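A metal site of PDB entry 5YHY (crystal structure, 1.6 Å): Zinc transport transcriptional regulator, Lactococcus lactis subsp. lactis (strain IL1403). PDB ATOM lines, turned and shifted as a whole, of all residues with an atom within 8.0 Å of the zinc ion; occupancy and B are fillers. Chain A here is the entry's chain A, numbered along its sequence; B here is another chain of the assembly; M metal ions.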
ATOM      1  N   HIS A  23       7.712 -23.069  25.724  1.00  0.00           N
ATOM      2  CA  HIS A  23       6.418 -23.453  25.166  1.00  0.00           C
ATOM      3  C   HIS A  23       5.605 -22.222  24.819  1.00  0.00           C
ATOM      4  O   HIS A  23       4.725 -22.278  23.971  1.00  0.00           O
ATOM      5  CB  HIS A  23       5.606 -24.270  26.179  1.00  0.00           C
ATOM      6  CG  HIS A  23       6.037 -25.692  26.300  1.00  0.00           C
ATOM      7  ND1 HIS A  23       6.312 -26.489  25.202  1.00  0.00           N
ATOM      8  CD2 HIS A  23       6.235 -26.472  27.389  1.00  0.00           C
ATOM      9  CE1 HIS A  23       6.659 -27.693  25.618  1.00  0.00           C
ATOM     10  NE2 HIS A  23       6.625 -27.706  26.938  1.00  0.00           N
ATOM     11  N   GLU A  24       5.899 -21.114  25.496  1.00  0.00           N
ATOM     12  CA  GLU A  24       5.118 -19.893  25.379  1.00  0.00           C
ATOM     13  C   GLU A  24       6.012 -18.691  25.594  1.00  0.00           C
ATOM     14  O   GLU A  24       6.968 -18.753  26.376  1.00  0.00           O
ATOM     15  CB  GLU A  24       4.022 -19.858  26.449  1.00  0.00           C
ATOM     16  CG  GLU A  24       2.698 -20.438  26.033  1.00  0.00           C
ATOM     17  CD  GLU A  24       1.612 -20.148  27.045  1.00  0.00           C
ATOM     18  OE1 GLU A  24       1.794 -20.489  28.236  1.00  0.00           O
ATOM     19  OE2 GLU A  24       0.570 -19.561  26.665  1.00  0.00           O
ATOM     20  N   ILE A  25       5.709 -17.594  24.919  1.00  0.00           N
ATOM     21  CA  ILE A  25       6.406 -16.341  25.185  1.00  0.00           C
ATOM     22  C   ILE A  25       5.772 -15.660  26.393  1.00  0.00           C
ATOM     23  O   ILE A  25       4.662 -15.121  26.314  1.00  0.00           O
ATOM     24  CB  ILE A  25       6.360 -15.392  23.964  1.00  0.00           C
ATOM     25  CG1 ILE A  25       7.056 -16.039  22.763  1.00  0.00           C
ATOM     26  CG2 ILE A  25       7.022 -14.057  24.302  1.00  0.00           C
ATOM     27  CD1 ILE A  25       8.527 -16.249  22.961  1.00  0.00           C
ATOM     28  N   LEU A  26       6.464 -15.695  27.526  1.00  0.00           N
ATOM     29  CA  LEU A  26       5.972 -15.092  28.759  1.00  0.00           C
ATOM     30  C   LEU A  26       7.061 -14.236  29.382  1.00  0.00           C
ATOM     31  O   LEU A  26       8.230 -14.644  29.422  1.00  0.00           O
ATOM     32  CB  LEU A  26       5.544 -16.167  29.755  1.00  0.00           C
ATOM     33  CG  LEU A  26       4.326 -16.974  29.320  1.00  0.00           C
ATOM     34  CD1 LEU A  26       4.150 -18.200  30.216  1.00  0.00           C
ATOM     35  CD2 LEU A  26       3.076 -16.110  29.338  1.00  0.00           C
ATOM     36  N   LYS A  29       9.179 -13.916  33.988  1.00  0.00           N
ATOM     37  CA  LYS A  29       9.330 -15.279  34.456  1.00  0.00           C
ATOM     38  C   LYS A  29      10.806 -15.668  34.455  1.00  0.00           C
ATOM     39  O   LYS A  29      11.520 -15.409  33.487  1.00  0.00           O
ATOM     40  CB  LYS A  29       8.543 -16.227  33.540  1.00  0.00           C
ATOM     41  CG  LYS A  29       8.666 -17.691  33.895  1.00  0.00           C
ATOM     42  CD  LYS A  29       7.755 -18.523  33.015  1.00  0.00           C
ATOM     43  CE  LYS A  29       7.914 -20.007  33.292  1.00  0.00           C
ATOM     44  NZ  LYS A  29       6.973 -20.832  32.493  1.00  0.00           N
ATOM     45  N   THR A  37       3.125 -28.787  29.686  1.00  0.00           N
ATOM     46  CA  THR A  37       2.828 -28.207  28.387  1.00  0.00           C
ATOM     47  C   THR A  37       1.926 -27.004  28.616  1.00  0.00           C
ATOM     48  O   THR A  37       1.355 -26.868  29.695  1.00  0.00           O
ATOM     49  CB  THR A  37       2.097 -29.186  27.476  1.00  0.00           C
ATOM     50  OG1 THR A  37       0.803 -29.464  28.029  1.00  0.00           O
ATOM     51  CG2 THR A  37       2.871 -30.480  27.337  1.00  0.00           C
ATOM     52  N   SER A  38       1.797 -26.155  27.603  1.00  0.00           N
ATOM     53  CA  SER A  38       0.934 -24.998  27.739  1.00  0.00           C
ATOM     54  C   SER A  38      -0.527 -25.412  27.938  1.00  0.00           C
ATOM     55  O   SER A  38      -1.224 -24.821  28.754  1.00  0.00           O
ATOM     56  CB  SER A  38       1.096 -24.057  26.530  1.00  0.00           C
ATOM     57  OG  SER A  38       0.724 -24.698  25.334  1.00  0.00           O
ATOM     58  N   THR A  39      -0.978 -26.437  27.218  1.00  0.00           N
ATOM     59  CA  THR A  39      -2.353 -26.900  27.398  1.00  0.00           C
ATOM     60  C   THR A  39      -2.572 -27.345  28.849  1.00  0.00           C
ATOM     61  O   THR A  39      -3.583 -27.021  29.459  1.00  0.00           O
ATOM     62  CB  THR A  39      -2.705 -28.047  26.429  1.00  0.00           C
ATOM     63  OG1 THR A  39      -2.699 -27.550  25.091  1.00  0.00           O
ATOM     64  CG2 THR A  39      -4.092 -28.593  26.736  1.00  0.00           C
ATOM     65  N   GLN A  40      -1.612 -28.086  29.398  1.00  0.00           N
ATOM     66  CA  GLN A  40      -1.722 -28.519  30.785  1.00  0.00           C
ATOM     67  C   GLN A  40      -1.815 -27.327  31.736  1.00  0.00           C
ATOM     68  O   GLN A  40      -2.654 -27.303  32.630  1.00  0.00           O
ATOM     69  CB  GLN A  40      -0.562 -29.446  31.142  1.00  0.00           C
ATOM     70  CG  GLN A  40      -0.647 -30.763  30.382  1.00  0.00           C
ATOM     71  CD  GLN A  40       0.666 -31.496  30.259  1.00  0.00           C
ATOM     72  OE1 GLN A  40       1.637 -31.179  30.944  1.00  0.00           O
ATOM     73  NE2 GLN A  40       0.713 -32.482  29.364  1.00  0.00           N
ATOM     74  N   GLU A  41      -0.955 -26.322  31.515  1.00  0.00           N
ATOM     75  CA  GLU A  41      -0.959 -25.133  32.371  1.00  0.00           C
ATOM     76  C   GLU A  41      -2.298 -24.419  32.263  1.00  0.00           C
ATOM     77  O   GLU A  41      -2.819 -23.911  33.252  1.00  0.00           O
ATOM     78  CB  GLU A  41       0.161 -24.164  31.961  1.00  0.00           C
ATOM     79  CG  GLU A  41       1.576 -24.699  32.099  1.00  0.00           C
ATOM     80  CD  GLU A  41       2.200 -24.375  33.445  1.00  0.00           C
ATOM     81  OE1 GLU A  41       1.471 -24.053  34.391  1.00  0.00           O
ATOM     82  OE2 GLU A  41       3.450 -24.456  33.541  1.00  0.00           O
ATOM     83  N   HIS A  42      -2.856 -24.387  31.058  1.00  0.00           N
ATOM     84  CA  HIS A  42      -4.095 -23.658  30.850  1.00  0.00           C
ATOM     85  C   HIS A  42      -5.303 -24.366  31.420  1.00  0.00           C
ATOM     86  O   HIS A  42      -6.242 -23.716  31.872  1.00  0.00           O
ATOM     87  CB  HIS A  42      -4.258 -23.299  29.380  1.00  0.00           C
ATOM     88  CG  HIS A  42      -3.159 -22.431  28.879  1.00  0.00           C
ATOM     89  ND1 HIS A  42      -2.954 -22.194  27.528  1.00  0.00           N
ATOM     90  CD2 HIS A  42      -2.175 -21.767  29.524  1.00  0.00           C
ATOM     91  CE1 HIS A  42      -1.901 -21.406  27.382  1.00  0.00           C
ATOM     92  NE2 HIS A  42      -1.407 -21.130  28.578  1.00  0.00           N
ATOM     93  N   MET A  45      -5.237 -23.316  35.028  1.00  0.00           N
ATOM     94  CA  MET A  45      -5.801 -21.969  35.173  1.00  0.00           C
ATOM     95  C   MET A  45      -7.304 -21.967  35.100  1.00  0.00           C
ATOM     96  O   MET A  45      -7.972 -21.251  35.835  1.00  0.00           O
ATOM     97  CB  MET A  45      -5.232 -21.009  34.116  1.00  0.00           C
ATOM     98  CG  MET A  45      -3.834 -20.539  34.409  1.00  0.00           C
ATOM     99  SD  MET A  45      -3.203 -19.389  33.166  1.00  0.00           S
ATOM    100  CE  MET A  45      -4.432 -18.098  33.201  1.00  0.00           C
ATOM    101  N   HIS A 108       1.239 -19.437  36.887  1.00  0.00           N
ATOM    102  CA  HIS A 108       1.073 -19.291  35.448  1.00  0.00           C
ATOM    103  C   HIS A 108       0.150 -18.129  35.091  1.00  0.00           C
ATOM    104  O   HIS A 108       0.400 -17.406  34.127  1.00  0.00           O
ATOM    105  CB  HIS A 108       0.562 -20.573  34.791  1.00  0.00           C
ATOM    106  CG  HIS A 108       0.835 -20.633  33.326  1.00  0.00           C
ATOM    107  ND1 HIS A 108       2.082 -20.870  32.816  1.00  0.00           N
ATOM    108  CD2 HIS A 108       0.009 -20.455  32.260  1.00  0.00           C
ATOM    109  CE1 HIS A 108       2.024 -20.863  31.492  1.00  0.00           C
ATOM    110  NE2 HIS A 108       0.786 -20.597  31.142  1.00  0.00           N
ATOM    111  N   ALA A 109      -0.918 -17.959  35.867  1.00  0.00           N
ATOM    112  CA  ALA A 109      -1.832 -16.854  35.649  1.00  0.00           C
ATOM    113  C   ALA A 109      -1.067 -15.549  35.792  1.00  0.00           C
ATOM    114  O   ALA A 109      -1.230 -14.619  35.006  1.00  0.00           O
ATOM    115  CB  ALA A 109      -2.991 -16.907  36.622  1.00  0.00           C
ATOM    116  N   HIS A 111       2.102 -14.991  35.253  1.00  0.00           N
ATOM    117  CA  HIS A 111       2.962 -14.791  34.092  1.00  0.00           C
ATOM    118  C   HIS A 111       2.190 -14.205  32.916  1.00  0.00           C
ATOM    119  O   HIS A 111       2.652 -13.274  32.267  1.00  0.00           O
ATOM    120  CB  HIS A 111       3.634 -16.095  33.661  1.00  0.00           C
ATOM    121  CG  HIS A 111       4.590 -16.633  34.667  1.00  0.00           C
ATOM    122  ND1 HIS A 111       5.353 -15.827  35.488  1.00  0.00           N
ATOM    123  CD2 HIS A 111       4.924 -17.910  34.998  1.00  0.00           C
ATOM    124  CE1 HIS A 111       6.104 -16.577  36.281  1.00  0.00           C
ATOM    125  NE2 HIS A 111       5.860 -17.849  36.003  1.00  0.00           N
ATOM    126  N   HIS A 112       1.016 -14.755  32.634  1.00  0.00           N
ATOM    127  CA  HIS A 112       0.172 -14.191  31.581  1.00  0.00           C
ATOM    128  C   HIS A 112      -0.241 -12.757  31.869  1.00  0.00           C
ATOM    129  O   HIS A 112      -0.221 -11.911  30.980  1.00  0.00           O
ATOM    130  CB  HIS A 112      -1.066 -15.053  31.342  1.00  0.00           C
ATOM    131  CG  HIS A 112      -0.798 -16.210  30.441  1.00  0.00           C
ATOM    132  ND1 HIS A 112      -0.724 -16.069  29.068  1.00  0.00           N
ATOM    133  CD2 HIS A 112      -0.552 -17.508  30.698  1.00  0.00           C
ATOM    134  CE1 HIS A 112      -0.460 -17.242  28.527  1.00  0.00           C
ATOM    135  NE2 HIS A 112      -0.348 -18.132  29.494  1.00  0.00           N
ATOM    136  N   ASP B   9       0.557 -10.390  21.673  1.00  0.00           N
ATOM    137  CA  ASP B   9       0.710 -11.731  22.258  1.00  0.00           C
ATOM    138  C   ASP B   9       0.596 -12.801  21.186  1.00  0.00           C
ATOM    139  O   ASP B   9       1.434 -13.714  21.098  1.00  0.00           O
ATOM    140  CB  ASP B   9      -0.365 -11.913  23.331  1.00  0.00           C
ATOM    141  CG  ASP B   9      -0.118 -13.112  24.223  1.00  0.00           C
ATOM    142  OD1 ASP B   9       1.052 -13.412  24.544  1.00  0.00           O
ATOM    143  OD2 ASP B   9      -1.117 -13.754  24.623  1.00  0.00           O
HETATM  144 ZN    ZN M   1       0.197 -20.095  29.256  1.00  0.00          ZN
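A ring nitrogen (ND1) of His 42 sits close to the backbone carbonyl oxygen of Ser 38 (3.4 Å).
Four residues have an atom within 4 Å of the zinc ion: Glu 24, His 42, His 108 and His 112.
The zinc ion is bound by the side-chain carboxylate of Glu 24, a ring nitrogen (NE2) of His 42, a ring nitrogen (NE2) of His 108 and a ring nitrogen (NE2) of His 112.
The zinc ion has four donor atoms within binding distance.
Slightly farther from the zinc ion lies OE2 of Glu 24 (2.7 Å).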
